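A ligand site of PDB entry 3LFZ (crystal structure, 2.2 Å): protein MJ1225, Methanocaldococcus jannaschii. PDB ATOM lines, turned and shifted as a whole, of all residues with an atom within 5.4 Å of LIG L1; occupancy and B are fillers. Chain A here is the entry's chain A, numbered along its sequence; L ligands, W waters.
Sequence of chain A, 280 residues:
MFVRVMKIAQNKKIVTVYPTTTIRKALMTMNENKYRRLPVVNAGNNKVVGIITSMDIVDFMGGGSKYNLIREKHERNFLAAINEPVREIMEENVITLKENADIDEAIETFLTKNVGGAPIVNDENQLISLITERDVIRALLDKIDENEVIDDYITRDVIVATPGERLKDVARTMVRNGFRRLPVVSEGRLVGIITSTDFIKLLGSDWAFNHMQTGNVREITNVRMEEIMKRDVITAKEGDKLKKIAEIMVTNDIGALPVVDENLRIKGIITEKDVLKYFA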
ATOM      1  N   ASN A 114      -9.992   2.878  28.997  1.00  0.00           N
ATOM      2  CA  ASN A 114      -8.765   2.516  28.292  1.00  0.00           C
ATOM      3  C   ASN A 114      -7.666   1.964  29.204  1.00  0.00           C
ATOM      4  O   ASN A 114      -6.517   2.412  29.150  1.00  0.00           O
ATOM      5  CB  ASN A 114      -8.263   3.711  27.465  1.00  0.00           C
ATOM      6  CG  ASN A 114      -7.264   3.329  26.396  1.00  0.00           C
ATOM      7  OD1 ASN A 114      -7.288   2.211  25.875  1.00  0.00           O
ATOM      8  ND2 ASN A 114      -6.376   4.254  26.048  1.00  0.00           N
ATOM      9  N   GLU A 133      -8.021  -7.834  31.733  1.00  0.00           N
ATOM     10  CA  GLU A 133      -8.966  -8.241  30.705  1.00  0.00           C
ATOM     11  C   GLU A 133      -8.841  -9.733  30.391  1.00  0.00           C
ATOM     12  O   GLU A 133      -9.823 -10.386  30.056  1.00  0.00           O
ATOM     13  CB  GLU A 133      -8.749  -7.431  29.427  1.00  0.00           C
ATOM     14  CG  GLU A 133      -8.906  -5.933  29.614  1.00  0.00           C
ATOM     15  CD  GLU A 133      -8.544  -5.157  28.365  1.00  0.00           C
ATOM     16  OE1 GLU A 133      -9.385  -4.376  27.899  1.00  0.00           O
ATOM     17  OE2 GLU A 133      -7.409  -5.328  27.860  1.00  0.00           O
ATOM     18  N   THR A 155     -10.924  -3.936  14.709  1.00  0.00           N
ATOM     19  CA  THR A 155     -10.560  -2.537  14.552  1.00  0.00           C
ATOM     20  C   THR A 155      -9.964  -2.367  13.162  1.00  0.00           C
ATOM     21  O   THR A 155      -8.872  -2.851  12.885  1.00  0.00           O
ATOM     22  CB  THR A 155      -9.607  -2.047  15.671  1.00  0.00           C
ATOM     23  OG1 THR A 155     -10.311  -2.030  16.919  1.00  0.00           O
ATOM     24  CG2 THR A 155      -9.098  -0.646  15.384  1.00  0.00           C
ATOM     25  N   ASP A 157      -9.118   0.522  11.120  1.00  0.00           N
ATOM     26  CA  ASP A 157      -8.021   1.457  10.903  1.00  0.00           C
ATOM     27  C   ASP A 157      -6.827   1.096  11.782  1.00  0.00           C
ATOM     28  O   ASP A 157      -6.798   1.456  12.958  1.00  0.00           O
ATOM     29  CB  ASP A 157      -8.453   2.893  11.205  1.00  0.00           C
ATOM     30  CG  ASP A 157      -9.415   3.454  10.173  1.00  0.00           C
ATOM     31  OD1 ASP A 157     -10.128   2.665   9.512  1.00  0.00           O
ATOM     32  OD2 ASP A 157      -9.454   4.689  10.033  1.00  0.00           O
ATOM     33  N   VAL A 158      -5.849   0.400  11.216  1.00  0.00           N
ATOM     34  CA  VAL A 158      -4.693  -0.026  12.009  1.00  0.00           C
ATOM     35  C   VAL A 158      -3.564   0.986  11.960  1.00  0.00           C
ATOM     36  O   VAL A 158      -3.190   1.475  10.885  1.00  0.00           O
ATOM     37  CB  VAL A 158      -4.156  -1.410  11.568  1.00  0.00           C
ATOM     38  CG1 VAL A 158      -3.322  -2.025  12.689  1.00  0.00           C
ATOM     39  CG2 VAL A 158      -5.296  -2.339  11.208  1.00  0.00           C
ATOM     40  N   ILE A 159      -3.057   1.329  13.132  1.00  0.00           N
ATOM     41  CA  ILE A 159      -1.811   2.064  13.262  1.00  0.00           C
ATOM     42  C   ILE A 159      -0.687   1.030  13.236  1.00  0.00           C
ATOM     43  O   ILE A 159      -0.774  -0.024  13.880  1.00  0.00           O
ATOM     44  CB  ILE A 159      -1.778   2.912  14.556  1.00  0.00           C
ATOM     45  CG1 ILE A 159      -2.985   3.865  14.632  1.00  0.00           C
ATOM     46  CG2 ILE A 159      -0.464   3.676  14.675  1.00  0.00           C
ATOM     47  CD1 ILE A 159      -3.021   4.980  13.580  1.00  0.00           C
ATOM     48  N   VAL A 160       0.344   1.342  12.475  1.00  0.00           N
ATOM     49  CA  VAL A 160       1.278   0.328  12.020  1.00  0.00           C
ATOM     50  C   VAL A 160       2.707   0.853  12.102  1.00  0.00           C
ATOM     51  O   VAL A 160       2.929   2.065  12.119  1.00  0.00           O
ATOM     52  CB  VAL A 160       0.920  -0.079  10.559  1.00  0.00           C
ATOM     53  CG1 VAL A 160       1.832  -1.168  10.059  1.00  0.00           C
ATOM     54  CG2 VAL A 160      -0.529  -0.548  10.448  1.00  0.00           C
ATOM     55  N   GLY A 178      -1.454   5.247  22.335  1.00  0.00           N
ATOM     56  CA  GLY A 178      -1.810   4.377  23.461  1.00  0.00           C
ATOM     57  C   GLY A 178      -1.946   2.911  23.062  1.00  0.00           C
ATOM     58  O   GLY A 178      -2.726   2.176  23.658  1.00  0.00           O
ATOM     59  N   PHE A 179      -1.178   2.505  22.049  1.00  0.00           N
ATOM     60  CA  PHE A 179      -1.188   1.121  21.569  1.00  0.00           C
ATOM     61  C   PHE A 179       0.130   0.439  21.883  1.00  0.00           C
ATOM     62  O   PHE A 179       1.185   0.869  21.423  1.00  0.00           O
ATOM     63  CB  PHE A 179      -1.412   1.059  20.049  1.00  0.00           C
ATOM     64  CG  PHE A 179      -2.705   1.666  19.579  1.00  0.00           C
ATOM     65  CD1 PHE A 179      -3.875   1.531  20.321  1.00  0.00           C
ATOM     66  CD2 PHE A 179      -2.758   2.342  18.370  1.00  0.00           C
ATOM     67  CE1 PHE A 179      -5.070   2.081  19.870  1.00  0.00           C
ATOM     68  CE2 PHE A 179      -3.955   2.905  17.907  1.00  0.00           C
ATOM     69  CZ  PHE A 179      -5.110   2.768  18.663  1.00  0.00           C
ATOM     70  N   ARG A 180       0.077  -0.633  22.666  1.00  0.00           N
ATOM     71  CA  ARG A 180       1.275  -1.389  23.026  1.00  0.00           C
ATOM     72  C   ARG A 180       1.795  -2.262  21.883  1.00  0.00           C
ATOM     73  O   ARG A 180       2.988  -2.559  21.818  1.00  0.00           O
ATOM     74  CB  ARG A 180       1.016  -2.280  24.237  1.00  0.00           C
ATOM     75  CG  ARG A 180       0.413  -1.561  25.437  1.00  0.00           C
ATOM     76  CD  ARG A 180       0.419  -2.480  26.651  1.00  0.00           C
ATOM     77  NE  ARG A 180       1.558  -3.376  26.613  1.00  0.00           N
ATOM     78  CZ  ARG A 180       1.468  -4.707  26.584  1.00  0.00           C
ATOM     79  NH1 ARG A 180       0.276  -5.293  26.638  1.00  0.00           N
ATOM     80  NH2 ARG A 180       2.569  -5.438  26.534  1.00  0.00           N
ATOM     81  N   ARG A 181       0.906  -2.696  20.998  1.00  0.00           N
ATOM     82  CA  ARG A 181       1.336  -3.519  19.870  1.00  0.00           C
ATOM     83  C   ARG A 181       0.991  -2.951  18.520  1.00  0.00           C
ATOM     84  O   ARG A 181      -0.132  -2.504  18.274  1.00  0.00           O
ATOM     85  CB  ARG A 181       0.870  -4.973  19.954  1.00  0.00           C
ATOM     86  CG  ARG A 181      -0.415  -5.177  20.680  1.00  0.00           C
ATOM     87  CD  ARG A 181      -0.119  -5.588  22.089  1.00  0.00           C
ATOM     88  NE  ARG A 181      -1.355  -5.786  22.806  1.00  0.00           N
ATOM     89  CZ  ARG A 181      -1.421  -6.328  24.015  1.00  0.00           C
ATOM     90  NH1 ARG A 181      -0.303  -6.704  24.618  1.00  0.00           N
ATOM     91  NH2 ARG A 181      -2.592  -6.484  24.622  1.00  0.00           N
ATOM     92  N   LEU A 182       1.983  -2.989  17.652  1.00  0.00           N
ATOM     93  CA  LEU A 182       1.847  -2.524  16.298  1.00  0.00           C
ATOM     94  C   LEU A 182       2.176  -3.651  15.330  1.00  0.00           C
ATOM     95  O   LEU A 182       3.265  -4.226  15.403  1.00  0.00           O
ATOM     96  CB  LEU A 182       2.767  -1.312  16.058  1.00  0.00           C
ATOM     97  CG  LEU A 182       2.669  -0.134  17.033  1.00  0.00           C
ATOM     98  CD1 LEU A 182       3.655   0.950  16.659  1.00  0.00           C
ATOM     99  CD2 LEU A 182       1.250   0.431  17.097  1.00  0.00           C
ATOM    100  N   PRO A 183       1.227  -3.976  14.437  1.00  0.00           N
ATOM    101  CA  PRO A 183       1.583  -4.903  13.376  1.00  0.00           C
ATOM    102  C   PRO A 183       2.664  -4.248  12.531  1.00  0.00           C
ATOM    103  O   PRO A 183       2.633  -3.041  12.334  1.00  0.00           O
ATOM    104  CB  PRO A 183       0.285  -5.055  12.575  1.00  0.00           C
ATOM    105  CG  PRO A 183      -0.798  -4.457  13.436  1.00  0.00           C
ATOM    106  CD  PRO A 183      -0.132  -3.424  14.270  1.00  0.00           C
ATOM    107  N   GLY A 255      -2.376 -10.677  23.590  1.00  0.00           N
ATOM    108  CA  GLY A 255      -3.467  -9.745  23.714  1.00  0.00           C
ATOM    109  C   GLY A 255      -4.006  -9.216  22.407  1.00  0.00           C
ATOM    110  O   GLY A 255      -5.079  -8.638  22.378  1.00  0.00           O
ATOM    111  N   ALA A 256      -3.259  -9.422  21.324  1.00  0.00           N
ATOM    112  CA  ALA A 256      -3.612  -8.826  20.031  1.00  0.00           C
ATOM    113  C   ALA A 256      -3.215  -9.687  18.831  1.00  0.00           C
ATOM    114  O   ALA A 256      -2.083 -10.168  18.734  1.00  0.00           O
ATOM    115  CB  ALA A 256      -2.983  -7.442  19.909  1.00  0.00           C
ATOM    116  N   ILE A 269      -7.116  -5.308  13.204  1.00  0.00           N
ATOM    117  CA  ILE A 269      -6.477  -5.880  14.380  1.00  0.00           C
ATOM    118  C   ILE A 269      -7.598  -6.153  15.380  1.00  0.00           C
ATOM    119  O   ILE A 269      -8.587  -5.417  15.411  1.00  0.00           O
ATOM    120  CB  ILE A 269      -5.390  -4.929  14.980  1.00  0.00           C
ATOM    121  CG1 ILE A 269      -4.606  -5.614  16.117  1.00  0.00           C
ATOM    122  CG2 ILE A 269      -6.001  -3.587  15.436  1.00  0.00           C
ATOM    123  CD1 ILE A 269      -3.284  -4.951  16.452  1.00  0.00           C
ATOM    124  N   ILE A 270      -7.474  -7.226  16.147  1.00  0.00           N
ATOM    125  CA  ILE A 270      -8.420  -7.529  17.218  1.00  0.00           C
ATOM    126  C   ILE A 270      -7.657  -7.817  18.504  1.00  0.00           C
ATOM    127  O   ILE A 270      -6.637  -8.513  18.487  1.00  0.00           O
ATOM    128  CB  ILE A 270      -9.395  -8.697  16.840  1.00  0.00           C
ATOM    129  CG1 ILE A 270     -10.434  -8.915  17.949  1.00  0.00           C
ATOM    130  CG2 ILE A 270      -8.617  -9.977  16.492  1.00  0.00           C
ATOM    131  CD1 ILE A 270     -11.634  -9.754  17.532  1.00  0.00           C
ATOM    132  N   THR A 271      -8.133  -7.260  19.603  1.00  0.00           N
ATOM    133  CA  THR A 271      -7.429  -7.374  20.872  1.00  0.00           C
ATOM    134  C   THR A 271      -8.378  -7.859  21.968  1.00  0.00           C
ATOM    135  O   THR A 271      -9.570  -8.019  21.734  1.00  0.00           O
ATOM    136  CB  THR A 271      -6.755  -6.028  21.291  1.00  0.00           C
ATOM    137  OG1 THR A 271      -7.734  -5.122  21.796  1.00  0.00           O
ATOM    138  CG2 THR A 271      -6.023  -5.379  20.112  1.00  0.00           C
ATOM    139  N   GLU A 272      -7.829  -8.092  23.152  1.00  0.00           N
ATOM    140  CA  GLU A 272      -8.608  -8.554  24.304  1.00  0.00           C
ATOM    141  C   GLU A 272      -9.732  -7.586  24.662  1.00  0.00           C
ATOM    142  O   GLU A 272     -10.809  -8.021  25.086  1.00  0.00           O
ATOM    143  CB  GLU A 272      -7.715  -8.732  25.521  1.00  0.00           C
ATOM    144  CG  GLU A 272      -6.605  -9.740  25.335  1.00  0.00           C
ATOM    145  CD  GLU A 272      -5.774  -9.922  26.590  1.00  0.00           C
ATOM    146  OE1 GLU A 272      -5.341  -8.903  27.171  1.00  0.00           O
ATOM    147  OE2 GLU A 272      -5.573 -11.079  26.994  1.00  0.00           O
ATOM    148  N   LYS A 273      -9.473  -6.279  24.504  1.00  0.00           N
ATOM    149  CA  LYS A 273     -10.509  -5.286  24.784  1.00  0.00           C
ATOM    150  C   LYS A 273     -11.690  -5.441  23.824  1.00  0.00           C
ATOM    151  O   LYS A 273     -12.836  -5.322  24.232  1.00  0.00           O
ATOM    152  CB  LYS A 273      -9.961  -3.861  24.726  1.00  0.00           C
ATOM    153  CG  LYS A 273     -10.862  -2.839  25.428  1.00  0.00           C
ATOM    154  CD  LYS A 273     -10.351  -1.407  25.322  1.00  0.00           C
ATOM    155  CE  LYS A 273      -9.009  -1.218  26.020  1.00  0.00           C
ATOM    156  NZ  LYS A 273      -9.017  -1.651  27.447  1.00  0.00           N
ATOM    157  N   ASP A 274     -11.390  -5.707  22.553  1.00  0.00           N
ATOM    158  CA  ASP A 274     -12.428  -5.945  21.560  1.00  0.00           C
ATOM    159  C   ASP A 274     -13.261  -7.148  21.929  1.00  0.00           C
ATOM    160  O   ASP A 274     -14.490  -7.066  21.976  1.00  0.00           O
ATOM    161  CB  ASP A 274     -11.824  -6.146  20.173  1.00  0.00           C
ATOM    162  CG  ASP A 274     -11.060  -4.932  19.686  1.00  0.00           C
ATOM    163  OD1 ASP A 274     -11.528  -3.795  19.929  1.00  0.00           O
ATOM    164  OD2 ASP A 274      -9.989  -5.127  19.084  1.00  0.00           O
ATOM    165  N   LYS A 277     -16.050  -6.605  24.265  1.00  0.00           N
ATOM    166  CA  LYS A 277     -17.241  -5.884  23.787  1.00  0.00           C
ATOM    167  C   LYS A 277     -18.440  -6.813  23.626  1.00  0.00           C
ATOM    168  O   LYS A 277     -19.593  -6.359  23.652  1.00  0.00           O
ATOM    169  CB  LYS A 277     -16.953  -5.170  22.462  1.00  0.00           C
ATOM    170  CG  LYS A 277     -16.007  -3.986  22.578  1.00  0.00           C
ATOM    171  CD  LYS A 277     -15.452  -3.603  21.230  1.00  0.00           C
ATOM    172  CE  LYS A 277     -14.468  -2.450  21.359  1.00  0.00           C
ATOM    173  NZ  LYS A 277     -13.867  -2.091  20.047  1.00  0.00           N
HETATM  174  P1  LIG L   1      -3.167  -2.544  22.725  1.00  0.00           P
HETATM  175  O1  LIG L   1      -3.239  -3.946  23.188  1.00  0.00           O
HETATM  176  O2  LIG L   1      -2.256  -2.389  21.390  1.00  0.00           O
HETATM  177  O3  LIG L   1      -2.563  -1.478  23.795  1.00  0.00           O
HETATM  178  P2  LIG L   1      -5.860  -2.250  23.361  1.00  0.00           P
HETATM  179  O4  LIG L   1      -6.059  -3.684  23.691  1.00  0.00           O
HETATM  180  O5  LIG L   1      -5.603  -1.287  24.648  1.00  0.00           O
HETATM  181  O6  LIG L   1      -4.609  -1.997  22.365  1.00  0.00           O
HETATM  182  O7  LIG L   1      -7.093  -1.786  22.464  1.00  0.00           O
HETATM  183  C1  LIG L   1      -7.822  -0.569  22.527  1.00  0.00           C
HETATM  184  C2  LIG L   1      -8.506  -0.388  21.155  1.00  0.00           C
HETATM  185  O8  LIG L   1      -7.472   0.075  20.232  1.00  0.00           O
HETATM  186  C3  LIG L   1      -9.051  -1.708  20.584  1.00  0.00           C
HETATM  187  O9  LIG L   1     -10.273  -1.460  19.870  1.00  0.00           O
HETATM  188  C4  LIG L   1      -7.957  -2.158  19.625  1.00  0.00           C
HETATM  189  O10 LIG L   1      -8.480  -2.961  18.561  1.00  0.00           O
HETATM  190  C5  LIG L   1      -7.411  -0.831  19.095  1.00  0.00           C
HETATM  191  N1  LIG L   1      -5.998  -1.008  18.641  1.00  0.00           N
HETATM  192  C6  LIG L   1      -5.040  -1.711  19.257  1.00  0.00           C
HETATM  193  N2  LIG L   1      -3.905  -1.641  18.559  1.00  0.00           N
HETATM  194  C7  LIG L   1      -4.139  -0.898  17.483  1.00  0.00           C
HETATM  195  C8  LIG L   1      -3.360  -0.487  16.414  1.00  0.00           C
HETATM  196  N3  LIG L   1      -2.084  -0.840  16.311  1.00  0.00           N
HETATM  197  N4  LIG L   1      -3.929   0.296  15.472  1.00  0.00           N
HETATM  198  C9  LIG L   1      -5.200   0.664  15.556  1.00  0.00           C
HETATM  199  N5  LIG L   1      -5.968   0.276  16.571  1.00  0.00           N
HETATM  200  C10 LIG L   1      -5.464  -0.498  17.541  1.00  0.00           C
HETATM  201  P1  LG2 L   2      -3.453  -2.978  27.612  1.00  0.00           P
HETATM  202  O1  LG2 L   2      -2.844  -2.427  26.228  1.00  0.00           O
HETATM  203  O2  LG2 L   2      -4.925  -2.884  27.644  1.00  0.00           O
HETATM  204  O3  LG2 L   2      -2.945  -4.512  27.676  1.00  0.00           O
HETATM  205  P2  LG2 L   2      -3.172  -0.803  29.507  1.00  0.00           P
HETATM  206  O4  LG2 L   2      -3.764   0.133  28.520  1.00  0.00           O
HETATM  207  O5  LG2 L   2      -3.925  -1.152  30.719  1.00  0.00           O
HETATM  208  O6  LG2 L   2      -2.658  -2.164  28.783  1.00  0.00           O
HETATM  209  P3  LG2 L   2      -0.563   0.166  29.082  1.00  0.00           P
HETATM  210  O7  LG2 L   2       0.539  -0.766  29.407  1.00  0.00           O
HETATM  211  O8  LG2 L   2      -1.003   0.325  27.680  1.00  0.00           O
HETATM  212  O9  LG2 L   2      -1.791  -0.190  30.039  1.00  0.00           O
HETATM  213  O10 LG2 L   2      -0.128   1.605  29.671  1.00  0.00           O
HETATM  214  C1  LG2 L   2      -0.646   2.856  29.180  1.00  0.00           C
HETATM  215  C2  LG2 L   2      -0.649   3.892  30.315  1.00  0.00           C
HETATM  216  O11 LG2 L   2      -1.768   3.557  31.184  1.00  0.00           O
HETATM  217  C3  LG2 L   2       0.623   3.811  31.173  1.00  0.00           C
HETATM  218  O12 LG2 L   2       1.076   5.137  31.460  1.00  0.00           O
HETATM  219  C4  LG2 L   2       0.156   3.094  32.441  1.00  0.00           C
HETATM  220  O13 LG2 L   2       0.912   3.498  33.585  1.00  0.00           O
HETATM  221  C5  LG2 L   2      -1.296   3.575  32.545  1.00  0.00           C
HETATM  222  N1  LG2 L   2      -2.136   2.629  33.313  1.00  0.00           N
HETATM  223  C6  LG2 L   2      -2.245   1.302  33.127  1.00  0.00           C
HETATM  224  N2  LG2 L   2      -3.098   0.793  34.009  1.00  0.00           N
HETATM  225  C7  LG2 L   2      -3.554   1.794  34.758  1.00  0.00           C
HETATM  226  C8  LG2 L   2      -4.454   1.879  35.813  1.00  0.00           C
HETATM  227  N3  LG2 L   2      -5.075   0.803  36.296  1.00  0.00           N
HETATM  228  N4  LG2 L   2      -4.701   3.090  36.361  1.00  0.00           N
HETATM  229  C9  LG2 L   2      -4.094   4.177  35.911  1.00  0.00           C
HETATM  230  N5  LG2 L   2      -3.225   4.128  34.908  1.00  0.00           N
HETATM  231  C10 LG2 L   2      -2.947   2.951  34.317  1.00  0.00           C
HETATM  232  O   HOH W   1      -6.718  -3.845  26.044  1.00  0.00           O
HETATM  233  O   HOH W   2      -8.319   2.740  22.457  1.00  0.00           O
HETATM  234  O   HOH W   3      -6.203  -0.601  27.553  1.00  0.00           O
HETATM  235  O   HOH W   4      -8.888   2.799  19.202  1.00  0.00           O
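Asp 157 touches LIG L1.
Val 158 touches LIG L1 (CA to N4, 3.6 Å).
Gly 178 touches LIG L1.
CE1 of Phe 179 touches O8 of LIG L1 (3.2 Å).
CD2 of Leu 182 touches N3 of LIG L1 (3.7 Å).
CD of Pro 183 touches N3 of LIG L1, 3.8 Å away.
CG2 of Ile 269 touches C10 of LIG L1 (3.8 Å).
Lys 273 touches LIG L1.
Lys 277 touches LIG L1 (NZ to O9, 3.7 Å).
15 residues have an atom within 4 Å of LIG L1: Thr 155, Asp 157, Val 158, Ile 159, Gly 178, Phe 179, Arg 180, Arg 181, Leu 182, Pro 183, Ile 269, Thr 271, Lys 273, Asp 274 and Lys 277.
The nearest printed residue that does not touch LIG L1 is Asn 114 (4.1 Å).
The backbone NH of Thr 155 lies within hydrogen-bond range of the backbone carbonyl oxygen of Ile 269.
The side-chain carboxylate (OD2) of Asp 274 sits at hydrogen-bond distance from the backbone NH (N) of Thr 271 (2.9 Å).
The side-chain amino group (NZ) of Lys 277 lies within salt-bridge range of the side-chain carboxylate (OD1) of Asp 274 (2.9 Å).
NH1 of Arg 180 lies close to NH1 of Arg 181.
The side-chain hydroxyl (OG1) of Thr 271 lies close to the backbone NH (N) of Lys 273, 3.4 Å away.
NZ of Lys 273 is in salt-bridge range of OE1 of Glu 133 (2.8 Å).
Water W1 lies within hydrogen-bond range of OE2 of Glu 133 (2.4 Å), O4 of LIG L1 (2.4 Å), O2 of LG2 L2 (2.6 Å) and NZ of Lys 273 (3.5 Å).
Water W3 lies within hydrogen-bond range of O2 of LG2 L2 (2.6 Å), NZ of Lys 273 (3.0 Å), O5 of LIG L1 (3.0 Å) and O of Asn 114 (3.4 Å).
O3 of LIG L1 lies close to O1 of LG2 L2 (2.6 Å).
The side-chain hydroxyl (OG1) of Thr 155 lies within hydrogen-bond range of an oxygen (O10) of LIG L1 (2.6 Å).
OD1 of Asp 274 sits at hydrogen-bond distance from O9 of LIG L1, 2.7 Å away.
The backbone NH (N) of Arg 181 is in hydrogen-bond range of an oxygen (O2) of LIG L1.
The backbone carbonyl oxygen (O) of Arg 181 is in hydrogen-bond range of a nitrogen (N3) of LIG L1, at 3.2 Å.
The guanidinium group (NE) of Arg 181 is in salt-bridge range of an oxygen (O1) of LIG L1, at 2.7 Å.
N of Ile 159 lies within hydrogen-bond range of N4 of LIG L1.
The backbone carbonyl oxygen of Ile 159 sits at hydrogen-bond distance from a nitrogen (N3) of LIG L1.
OG1 of Thr 271 is in hydrogen-bond range of O4 of LIG L1 (2.9 Å).
O3 of LIG L1 is in hydrogen-bond range of N of Arg 180, 3.0 Å away.
NH2 of Arg 181 lies within salt-bridge range of O3 of LG2 L2 (3.7 Å).
The guanidinium group (NH1) of Arg 180 is in salt-bridge range of an oxygen (O3) of LG2 L2.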
